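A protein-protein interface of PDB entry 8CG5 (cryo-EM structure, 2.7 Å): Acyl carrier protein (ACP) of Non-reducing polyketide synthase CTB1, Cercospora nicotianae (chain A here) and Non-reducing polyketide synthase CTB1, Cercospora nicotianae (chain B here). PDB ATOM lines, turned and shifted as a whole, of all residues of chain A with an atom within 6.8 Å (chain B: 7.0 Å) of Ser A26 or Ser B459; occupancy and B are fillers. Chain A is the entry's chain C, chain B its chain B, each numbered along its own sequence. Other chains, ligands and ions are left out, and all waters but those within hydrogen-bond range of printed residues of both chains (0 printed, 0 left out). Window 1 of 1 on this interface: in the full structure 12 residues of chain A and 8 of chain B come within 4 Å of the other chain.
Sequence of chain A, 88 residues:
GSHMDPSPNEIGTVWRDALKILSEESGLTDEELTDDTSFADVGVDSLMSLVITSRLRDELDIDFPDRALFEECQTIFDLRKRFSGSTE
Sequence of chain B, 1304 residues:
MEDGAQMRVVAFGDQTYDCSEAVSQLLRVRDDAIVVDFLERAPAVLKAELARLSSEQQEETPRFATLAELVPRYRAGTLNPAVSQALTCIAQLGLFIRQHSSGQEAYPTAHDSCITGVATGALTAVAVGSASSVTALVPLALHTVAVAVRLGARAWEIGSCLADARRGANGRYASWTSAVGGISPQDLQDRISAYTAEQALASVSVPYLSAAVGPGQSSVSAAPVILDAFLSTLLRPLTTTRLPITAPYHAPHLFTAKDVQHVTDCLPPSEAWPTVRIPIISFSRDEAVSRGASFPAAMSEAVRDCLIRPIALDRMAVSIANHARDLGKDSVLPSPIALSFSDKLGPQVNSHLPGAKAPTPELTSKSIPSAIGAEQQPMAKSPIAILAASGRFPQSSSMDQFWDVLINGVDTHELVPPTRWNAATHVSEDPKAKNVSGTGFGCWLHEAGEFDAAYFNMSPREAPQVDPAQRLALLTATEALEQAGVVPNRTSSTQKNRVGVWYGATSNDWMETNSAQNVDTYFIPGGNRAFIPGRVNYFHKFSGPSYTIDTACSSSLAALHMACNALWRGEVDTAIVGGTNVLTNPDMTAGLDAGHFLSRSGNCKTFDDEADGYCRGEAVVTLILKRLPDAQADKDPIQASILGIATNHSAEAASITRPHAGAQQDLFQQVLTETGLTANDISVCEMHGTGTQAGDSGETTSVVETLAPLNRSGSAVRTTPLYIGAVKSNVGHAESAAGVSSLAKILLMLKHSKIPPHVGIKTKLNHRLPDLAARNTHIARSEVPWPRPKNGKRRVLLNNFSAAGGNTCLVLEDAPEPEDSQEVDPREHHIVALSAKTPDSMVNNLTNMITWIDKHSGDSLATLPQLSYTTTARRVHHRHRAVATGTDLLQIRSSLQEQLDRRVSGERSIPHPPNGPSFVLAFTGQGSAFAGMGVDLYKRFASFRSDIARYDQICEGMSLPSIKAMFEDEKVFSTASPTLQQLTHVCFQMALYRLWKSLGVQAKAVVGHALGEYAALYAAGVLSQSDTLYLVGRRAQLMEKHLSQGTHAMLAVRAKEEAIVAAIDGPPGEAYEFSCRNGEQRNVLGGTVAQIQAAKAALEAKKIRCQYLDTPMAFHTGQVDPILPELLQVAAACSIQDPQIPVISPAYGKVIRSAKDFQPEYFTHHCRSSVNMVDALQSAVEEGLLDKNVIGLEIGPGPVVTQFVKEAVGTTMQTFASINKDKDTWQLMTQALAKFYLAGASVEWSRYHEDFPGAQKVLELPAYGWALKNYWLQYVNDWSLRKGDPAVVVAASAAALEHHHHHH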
ATOM      1  N   ILE A  21      23.474  24.765   0.293  1.00  0.00           N
ATOM      2  CA  ILE A  21      23.505  25.568  -0.929  1.00  0.00           C
ATOM      3  C   ILE A  21      22.804  24.828  -2.062  1.00  0.00           C
ATOM      4  O   ILE A  21      22.008  25.405  -2.817  1.00  0.00           O
ATOM      5  CB  ILE A  21      24.960  25.909  -1.302  1.00  0.00           C
ATOM      6  CG1 ILE A  21      25.552  26.927  -0.323  1.00  0.00           C
ATOM      7  CG2 ILE A  21      25.038  26.430  -2.730  1.00  0.00           C
ATOM      8  CD1 ILE A  21      24.961  28.319  -0.418  1.00  0.00           C
ATOM      9  N   LEU A  22      23.109  23.538  -2.204  1.00  0.00           N
ATOM     10  CA  LEU A  22      22.508  22.741  -3.267  1.00  0.00           C
ATOM     11  C   LEU A  22      21.000  22.645  -3.091  1.00  0.00           C
ATOM     12  O   LEU A  22      20.249  22.752  -4.065  1.00  0.00           O
ATOM     13  CB  LEU A  22      23.134  21.348  -3.293  1.00  0.00           C
ATOM     14  CG  LEU A  22      22.783  20.491  -4.509  1.00  0.00           C
ATOM     15  CD1 LEU A  22      23.614  20.910  -5.706  1.00  0.00           C
ATOM     16  CD2 LEU A  22      22.987  19.017  -4.204  1.00  0.00           C
ATOM     17  N   SER A  23      20.535  22.437  -1.857  1.00  0.00           N
ATOM     18  CA  SER A  23      19.099  22.364  -1.617  1.00  0.00           C
ATOM     19  C   SER A  23      18.426  23.696  -1.915  1.00  0.00           C
ATOM     20  O   SER A  23      17.323  23.730  -2.475  1.00  0.00           O
ATOM     21  CB  SER A  23      18.830  21.935  -0.175  1.00  0.00           C
ATOM     22  OG  SER A  23      18.903  23.042   0.705  1.00  0.00           O
ATOM     23  N   GLU A  24      19.067  24.807  -1.547  1.00  0.00           N
ATOM     24  CA  GLU A  24      18.498  26.116  -1.852  1.00  0.00           C
ATOM     25  C   GLU A  24      18.354  26.309  -3.355  1.00  0.00           C
ATOM     26  O   GLU A  24      17.283  26.683  -3.845  1.00  0.00           O
ATOM     27  CB  GLU A  24      19.365  27.229  -1.261  1.00  0.00           C
ATOM     28  CG  GLU A  24      18.995  27.627   0.162  1.00  0.00           C
ATOM     29  CD  GLU A  24      20.175  27.618   1.118  1.00  0.00           C
ATOM     30  OE1 GLU A  24      21.330  27.500   0.658  1.00  0.00           O
ATOM     31  OE2 GLU A  24      19.943  27.739   2.339  1.00  0.00           O
ATOM     32  N   GLU A  25      19.430  26.065  -4.104  1.00  0.00           N
ATOM     33  CA  GLU A  25      19.385  26.317  -5.540  1.00  0.00           C
ATOM     34  C   GLU A  25      18.471  25.333  -6.262  1.00  0.00           C
ATOM     35  O   GLU A  25      17.831  25.700  -7.254  1.00  0.00           O
ATOM     36  CB  GLU A  25      20.794  26.267  -6.125  1.00  0.00           C
ATOM     37  CG  GLU A  25      21.713  27.364  -5.610  1.00  0.00           C
ATOM     38  CD  GLU A  25      21.292  28.746  -6.072  1.00  0.00           C
ATOM     39  OE1 GLU A  25      20.316  28.847  -6.845  1.00  0.00           O
ATOM     40  OE2 GLU A  25      21.933  29.733  -5.660  1.00  0.00           O
ATOM     41  N   SER A  26      18.396  24.091  -5.789  1.00  0.00           N
ATOM     42  CA  SER A  26      17.543  23.080  -6.396  1.00  0.00           C
ATOM     43  C   SER A  26      16.105  23.142  -5.909  1.00  0.00           C
ATOM     44  O   SER A  26      15.214  22.628  -6.592  1.00  0.00           O
ATOM     45  CB  SER A  26      18.089  21.681  -6.100  1.00  0.00           C
ATOM     46  OG  SER A  26      18.930  21.199  -7.130  1.00  0.00           O
ATOM     47  N   GLY A  27      15.861  23.751  -4.754  1.00  0.00           N
ATOM     48  CA  GLY A  27      14.531  23.735  -4.176  1.00  0.00           C
ATOM     49  C   GLY A  27      14.055  22.356  -3.777  1.00  0.00           C
ATOM     50  O   GLY A  27      12.854  22.079  -3.854  1.00  0.00           O
ATOM     51  N   LEU A  28      14.964  21.483  -3.344  1.00  0.00           N
ATOM     52  CA  LEU A  28      14.614  20.147  -2.893  1.00  0.00           C
ATOM     53  C   LEU A  28      14.640  20.083  -1.367  1.00  0.00           C
ATOM     54  O   LEU A  28      14.830  21.089  -0.677  1.00  0.00           O
ATOM     55  CB  LEU A  28      15.545  19.098  -3.511  1.00  0.00           C
ATOM     56  CG  LEU A  28      15.602  18.962  -5.036  1.00  0.00           C
ATOM     57  CD1 LEU A  28      15.832  17.519  -5.454  1.00  0.00           C
ATOM     58  CD2 LEU A  28      14.347  19.490  -5.688  1.00  0.00           C
ATOM     59  N   LEU A  33      17.529  14.426  -1.716  1.00  0.00           N
ATOM     60  CA  LEU A  33      18.860  14.788  -2.204  1.00  0.00           C
ATOM     61  C   LEU A  33      19.913  13.952  -1.472  1.00  0.00           C
ATOM     62  O   LEU A  33      20.803  14.458  -0.788  1.00  0.00           O
ATOM     63  CB  LEU A  33      19.111  16.282  -2.026  1.00  0.00           C
ATOM     64  CG  LEU A  33      18.772  17.216  -3.190  1.00  0.00           C
ATOM     65  CD1 LEU A  33      19.099  18.651  -2.816  1.00  0.00           C
ATOM     66  CD2 LEU A  33      19.510  16.828  -4.463  1.00  0.00           C
ATOM     67  N   PHE A  39      22.157  13.656 -10.576  1.00  0.00           N
ATOM     68  CA  PHE A  39      21.976  15.070 -10.891  1.00  0.00           C
ATOM     69  C   PHE A  39      21.056  15.272 -12.088  1.00  0.00           C
ATOM     70  O   PHE A  39      20.385  16.306 -12.184  1.00  0.00           O
ATOM     71  CB  PHE A  39      23.329  15.729 -11.151  1.00  0.00           C
ATOM     72  CG  PHE A  39      24.073  16.101  -9.900  1.00  0.00           C
ATOM     73  CD1 PHE A  39      23.706  17.217  -9.167  1.00  0.00           C
ATOM     74  CD2 PHE A  39      25.150  15.350  -9.469  1.00  0.00           C
ATOM     75  CE1 PHE A  39      24.389  17.564  -8.022  1.00  0.00           C
ATOM     76  CE2 PHE A  39      25.838  15.696  -8.325  1.00  0.00           C
ATOM     77  CZ  PHE A  39      25.458  16.804  -7.602  1.00  0.00           C
ATOM     78  N   ASP A  41      18.301  13.447 -12.893  1.00  0.00           N
ATOM     79  CA  ASP A  41      16.913  13.332 -12.462  1.00  0.00           C
ATOM     80  C   ASP A  41      16.482  14.550 -11.655  1.00  0.00           C
ATOM     81  O   ASP A  41      15.329  14.984 -11.744  1.00  0.00           O
ATOM     82  CB  ASP A  41      16.723  12.054 -11.649  1.00  0.00           C
ATOM     83  CG  ASP A  41      17.152  10.816 -12.407  1.00  0.00           C
ATOM     84  OD1 ASP A  41      17.379  10.917 -13.631  1.00  0.00           O
ATOM     85  OD2 ASP A  41      17.260   9.740 -11.781  1.00  0.00           O
ATOM     86  N   VAL A  42      17.395  15.111 -10.860  1.00  0.00           N
ATOM     87  CA  VAL A  42      17.075  16.319 -10.104  1.00  0.00           C
ATOM     88  C   VAL A  42      16.655  17.431 -11.052  1.00  0.00           C
ATOM     89  O   VAL A  42      15.737  18.206 -10.758  1.00  0.00           O
ATOM     90  CB  VAL A  42      18.278  16.739  -9.240  1.00  0.00           C
ATOM     91  CG1 VAL A  42      18.177  18.212  -8.839  1.00  0.00           C
ATOM     92  CG2 VAL A  42      18.383  15.857  -8.014  1.00  0.00           C
ATOM     93  N   GLY A  43      17.318  17.528 -12.196  1.00  0.00           N
ATOM     94  CA  GLY A  43      17.071  18.585 -13.143  1.00  0.00           C
ATOM     95  C   GLY A  43      18.090  19.699 -13.130  1.00  0.00           C
ATOM     96  O   GLY A  43      17.741  20.834 -13.470  1.00  0.00           O
ATOM     97  N   VAL A  44      19.330  19.418 -12.743  1.00  0.00           N
ATOM     98  CA  VAL A  44      20.391  20.418 -12.758  1.00  0.00           C
ATOM     99  C   VAL A  44      21.044  20.380 -14.135  1.00  0.00           C
ATOM    100  O   VAL A  44      21.624  19.367 -14.536  1.00  0.00           O
ATOM    101  CB  VAL A  44      21.410  20.184 -11.634  1.00  0.00           C
ATOM    102  CG1 VAL A  44      20.697  19.828 -10.342  1.00  0.00           C
ATOM    103  CG2 VAL A  44      22.407  19.096 -11.999  1.00  0.00           C
ATOM    104  N   MET A  48      22.393  25.702 -14.417  1.00  0.00           N
ATOM    105  CA  MET A  48      22.212  25.774 -12.973  1.00  0.00           C
ATOM    106  C   MET A  48      23.480  25.375 -12.230  1.00  0.00           C
ATOM    107  O   MET A  48      23.786  25.940 -11.172  1.00  0.00           O
ATOM    108  CB  MET A  48      21.038  24.886 -12.568  1.00  0.00           C
ATOM    109  CG  MET A  48      20.877  24.650 -11.083  1.00  0.00           C
ATOM    110  SD  MET A  48      19.767  23.270 -10.805  1.00  0.00           S
ATOM    111  CE  MET A  48      19.596  23.336  -9.037  1.00  0.00           C
ATOM    112  N   ILE A  52      25.462  27.160  -9.095  1.00  0.00           N
ATOM    113  CA  ILE A  52      25.878  26.436  -7.896  1.00  0.00           C
ATOM    114  C   ILE A  52      27.360  26.666  -7.637  1.00  0.00           C
ATOM    115  O   ILE A  52      27.763  27.041  -6.530  1.00  0.00           O
ATOM    116  CB  ILE A  52      25.555  24.935  -8.025  1.00  0.00           C
ATOM    117  CG1 ILE A  52      24.170  24.626  -7.457  1.00  0.00           C
ATOM    118  CG2 ILE A  52      26.590  24.085  -7.298  1.00  0.00           C
ATOM    119  CD1 ILE A  52      23.043  25.275  -8.202  1.00  0.00           C
ATOM    120  N   ALA B 453       6.864  17.653 -12.446  1.00  0.00           N
ATOM    121  CA  ALA B 453       8.249  18.053 -12.666  1.00  0.00           C
ATOM    122  C   ALA B 453       9.184  16.851 -12.689  1.00  0.00           C
ATOM    123  O   ALA B 453      10.075  16.766 -13.539  1.00  0.00           O
ATOM    124  CB  ALA B 453       8.681  19.045 -11.589  1.00  0.00           C
ATOM    125  N   ALA B 454       8.995  15.908 -11.765  1.00  0.00           N
ATOM    126  CA  ALA B 454       9.912  14.778 -11.668  1.00  0.00           C
ATOM    127  C   ALA B 454       9.914  13.955 -12.949  1.00  0.00           C
ATOM    128  O   ALA B 454      10.965  13.473 -13.385  1.00  0.00           O
ATOM    129  CB  ALA B 454       9.539  13.905 -10.473  1.00  0.00           C
ATOM    130  N   PHE B 456       9.514  14.963 -15.982  1.00  0.00           N
ATOM    131  CA  PHE B 456      10.181  15.682 -17.057  1.00  0.00           C
ATOM    132  C   PHE B 456      11.530  16.252 -16.631  1.00  0.00           C
ATOM    133  O   PHE B 456      11.995  17.241 -17.204  1.00  0.00           O
ATOM    134  CB  PHE B 456       9.272  16.790 -17.582  1.00  0.00           C
ATOM    135  CG  PHE B 456       8.047  16.277 -18.278  1.00  0.00           C
ATOM    136  CD1 PHE B 456       8.127  15.776 -19.563  1.00  0.00           C
ATOM    137  CD2 PHE B 456       6.822  16.275 -17.643  1.00  0.00           C
ATOM    138  CE1 PHE B 456       7.010  15.298 -20.203  1.00  0.00           C
ATOM    139  CE2 PHE B 456       5.701  15.797 -18.281  1.00  0.00           C
ATOM    140  CZ  PHE B 456       5.797  15.307 -19.562  1.00  0.00           C
ATOM    141  N   ASN B 457      12.166  15.645 -15.630  1.00  0.00           N
ATOM    142  CA  ASN B 457      13.534  15.991 -15.253  1.00  0.00           C
ATOM    143  C   ASN B 457      13.676  17.485 -14.988  1.00  0.00           C
ATOM    144  O   ASN B 457      14.660  18.116 -15.375  1.00  0.00           O
ATOM    145  CB  ASN B 457      14.518  15.538 -16.329  1.00  0.00           C
ATOM    146  CG  ASN B 457      14.432  14.056 -16.608  1.00  0.00           C
ATOM    147  OD1 ASN B 457      14.154  13.259 -15.714  1.00  0.00           O
ATOM    148  ND2 ASN B 457      14.670  13.674 -17.856  1.00  0.00           N
ATOM    149  N   MET B 458      12.683  18.057 -14.323  1.00  0.00           N
ATOM    150  CA  MET B 458      12.699  19.459 -13.946  1.00  0.00           C
ATOM    151  C   MET B 458      12.980  19.571 -12.450  1.00  0.00           C
ATOM    152  O   MET B 458      13.138  18.573 -11.744  1.00  0.00           O
ATOM    153  CB  MET B 458      11.374  20.121 -14.322  1.00  0.00           C
ATOM    154  CG  MET B 458      11.441  21.632 -14.458  1.00  0.00           C
ATOM    155  SD  MET B 458      10.406  22.315 -15.769  1.00  0.00           S
ATOM    156  CE  MET B 458      10.935  21.377 -17.197  1.00  0.00           C
ATOM    157  N   SER B 459      13.043  20.802 -11.959  1.00  0.00           N
ATOM    158  CA  SER B 459      13.298  21.055 -10.552  1.00  0.00           C
ATOM    159  C   SER B 459      12.239  21.991  -9.993  1.00  0.00           C
ATOM    160  O   SER B 459      11.686  22.817 -10.725  1.00  0.00           O
ATOM    161  CB  SER B 459      14.687  21.672 -10.345  1.00  0.00           C
ATOM    162  OG  SER B 459      14.635  23.082 -10.450  1.00  0.00           O
ATOM    163  N   PRO B 460      11.938  21.888  -8.697  1.00  0.00           N
ATOM    164  CA  PRO B 460      10.902  22.756  -8.121  1.00  0.00           C
ATOM    165  C   PRO B 460      11.165  24.233  -8.324  1.00  0.00           C
ATOM    166  O   PRO B 460      10.208  25.009  -8.421  1.00  0.00           O
ATOM    167  CB  PRO B 460      10.925  22.386  -6.634  1.00  0.00           C
ATOM    168  CG  PRO B 460      11.445  21.009  -6.585  1.00  0.00           C
ATOM    169  CD  PRO B 460      12.310  20.792  -7.791  1.00  0.00           C
ATOM    170  N   ARG B 461      12.428  24.657  -8.367  1.00  0.00           N
ATOM    171  CA  ARG B 461      12.714  26.064  -8.609  1.00  0.00           C
ATOM    172  C   ARG B 461      12.674  26.402 -10.092  1.00  0.00           C
ATOM    173  O   ARG B 461      12.357  27.540 -10.454  1.00  0.00           O
ATOM    174  CB  ARG B 461      14.074  26.438  -8.024  1.00  0.00           C
ATOM    175  CG  ARG B 461      14.229  27.929  -7.792  1.00  0.00           C
ATOM    176  CD  ARG B 461      15.550  28.274  -7.133  1.00  0.00           C
ATOM    177  NE  ARG B 461      16.062  29.559  -7.595  1.00  0.00           N
ATOM    178  CZ  ARG B 461      16.659  30.460  -6.826  1.00  0.00           C
ATOM    179  NH1 ARG B 461      16.852  30.251  -5.533  1.00  0.00           N
ATOM    180  NH2 ARG B 461      17.073  31.601  -7.367  1.00  0.00           N
ATOM    181  N   GLU B 462      12.990  25.440 -10.958  1.00  0.00           N
ATOM    182  CA  GLU B 462      12.928  25.689 -12.393  1.00  0.00           C
ATOM    183  C   GLU B 462      11.491  25.682 -12.897  1.00  0.00           C
ATOM    184  O   GLU B 462      11.145  26.440 -13.809  1.00  0.00           O
ATOM    185  CB  GLU B 462      13.760  24.644 -13.135  1.00  0.00           C
ATOM    186  CG  GLU B 462      13.461  24.537 -14.621  1.00  0.00           C
ATOM    187  CD  GLU B 462      14.411  23.598 -15.336  1.00  0.00           C
ATOM    188  OE1 GLU B 462      15.088  22.804 -14.653  1.00  0.00           O
ATOM    189  OE2 GLU B 462      14.480  23.651 -16.582  1.00  0.00           O
ATOM    190  N   ALA B 463      10.640  24.838 -12.315  1.00  0.00           N
ATOM    191  CA  ALA B 463       9.296  24.648 -12.857  1.00  0.00           C
ATOM    192  C   ALA B 463       8.472  25.925 -12.869  1.00  0.00           C
ATOM    193  O   ALA B 463       7.924  26.268 -13.930  1.00  0.00           O
ATOM    194  CB  ALA B 463       8.585  23.544 -12.072  1.00  0.00           C
ATOM    195  N   PRO B 464       8.341  26.675 -11.771  1.00  0.00           N
ATOM    196  CA  PRO B 464       7.515  27.893 -11.818  1.00  0.00           C
ATOM    197  C   PRO B 464       8.039  28.933 -12.784  1.00  0.00           C
ATOM    198  O   PRO B 464       7.309  29.881 -13.099  1.00  0.00           O
ATOM    199  CB  PRO B 464       7.548  28.404 -10.372  1.00  0.00           C
ATOM    200  CG  PRO B 464       8.695  27.733  -9.736  1.00  0.00           C
ATOM    201  CD  PRO B 464       8.876  26.427 -10.426  1.00  0.00           C
ATOM    202  N   GLN B 465       9.273  28.793 -13.257  1.00  0.00           N
ATOM    203  CA  GLN B 465       9.854  29.720 -14.215  1.00  0.00           C
ATOM    204  C   GLN B 465       9.539  29.361 -15.659  1.00  0.00           C
ATOM    205  O   GLN B 465       9.834  30.159 -16.554  1.00  0.00           O
ATOM    206  CB  GLN B 465      11.368  29.767 -14.035  1.00  0.00           C
ATOM    207  CG  GLN B 465      11.795  30.204 -12.659  1.00  0.00           C
ATOM    208  CD  GLN B 465      12.935  31.184 -12.705  1.00  0.00           C
ATOM    209  OE1 GLN B 465      14.047  30.879 -12.281  1.00  0.00           O
ATOM    210  NE2 GLN B 465      12.667  32.373 -13.234  1.00  0.00           N
ATOM    211  N   TYR B 522      16.339  30.980 -15.289  1.00  0.00           N
ATOM    212  CA  TYR B 522      15.539  30.308 -16.306  1.00  0.00           C
ATOM    213  C   TYR B 522      14.535  31.248 -16.963  1.00  0.00           C
ATOM    214  O   TYR B 522      13.479  30.812 -17.424  1.00  0.00           O
ATOM    215  CB  TYR B 522      14.822  29.104 -15.703  1.00  0.00           C
ATOM    216  CG  TYR B 522      15.755  27.993 -15.305  1.00  0.00           C
ATOM    217  CD1 TYR B 522      16.331  27.172 -16.262  1.00  0.00           C
ATOM    218  CD2 TYR B 522      16.066  27.766 -13.974  1.00  0.00           C
ATOM    219  CE1 TYR B 522      17.186  26.156 -15.905  1.00  0.00           C
ATOM    220  CE2 TYR B 522      16.923  26.750 -13.608  1.00  0.00           C
ATOM    221  CZ  TYR B 522      17.480  25.950 -14.579  1.00  0.00           C
ATOM    222  OH  TYR B 522      18.331  24.934 -14.222  1.00  0.00           O
ATOM    223  N   TYR B1271       2.621  24.892  -9.843  1.00  0.00           N
ATOM    224  CA  TYR B1271       3.819  25.713 -10.006  1.00  0.00           C
ATOM    225  C   TYR B1271       3.387  27.030 -10.641  1.00  0.00           C
ATOM    226  O   TYR B1271       3.218  27.111 -11.860  1.00  0.00           O
ATOM    227  CB  TYR B1271       4.860  24.999 -10.858  1.00  0.00           C
ATOM    228  CG  TYR B1271       5.441  23.772 -10.203  1.00  0.00           C
ATOM    229  CD1 TYR B1271       6.239  23.877  -9.076  1.00  0.00           C
ATOM    230  CD2 TYR B1271       5.190  22.509 -10.710  1.00  0.00           C
ATOM    231  CE1 TYR B1271       6.770  22.760  -8.475  1.00  0.00           C
ATOM    232  CE2 TYR B1271       5.719  21.386 -10.116  1.00  0.00           C
ATOM    233  CZ  TYR B1271       6.507  21.518  -8.998  1.00  0.00           C
ATOM    234  OH  TYR B1271       7.037  20.402  -8.398  1.00  0.00           O
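The guanidinium group (NH1) of Arg B461 is in salt-bridge range of the side-chain carboxylate (OE1) of Glu A25 (3.96 Å).
O of Val A42 sits close to O of Met B458 (2.8 Å).
The backbone NH (N) of Arg B461 sits close to the side-chain hydroxyl (OG) of Ser B459 (3.4 Å).
OG of Ser B459 sits at hydrogen-bond distance from N of Glu B462 (2.9 Å).
The backbone carbonyl oxygen (O) of Ser A23 sits at hydrogen-bond distance from the backbone NH (N) of Leu A28 (3.4 Å).
OE1 of Glu A24 lies close to N of Ile A21.
The backbone carbonyl oxygen of Ala B453 sits at hydrogen-bond distance from the backbone NH of Met B458 (3.0 Å).
Among the printed residues, merely in contact across the chains: Glu A24 with Arg B461, Ser A26 with Ser B459, Ser A26 with Pro B460, Ser A26 with Arg B461, Gly A27 with Pro B460, Leu A28 with Pro B460, Val A42 with Ser B459, Gly A43 with Asn B457, Gly A43 with Glu B462 and Met A48 with Tyr B522.
Ser A23 touches none of the printed residues of chain B.
Ser A26 touches just these residues of chain B: Ser B459 (3.9 Å), Pro B460 (3.6 Å) and Arg B461 (3.9 Å).
Ala B454 touches none of the printed residues of chain A.
Of chain A, only Ser A26 and Val A42 come within 4 Å of Ser B459.
Printed residues of chain A within 4 Å of Arg B461: Glu A24 (3.97 Å), Glu A25 (3.4 Å) and Ser A26 (3.9 Å).
Of the printed residues of chain A, Tyr B522 touches Met A48 (3.2 Å).
The nearest residue of chain A that does not touch Ser B459 is Gly A43 (4.4 Å).
The nearest printed residue of chain A that does not touch Tyr B522 is Gly A43 (4.2 Å).
Of the 16 printed residues of chain A, 8 touch a printed residue of chain B.
Among the printed residues, Asp or Glu carboxylates within 4 Å of a Lys or Arg side-chain nitrogen of the other chain: Glu A25 with Arg B461.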
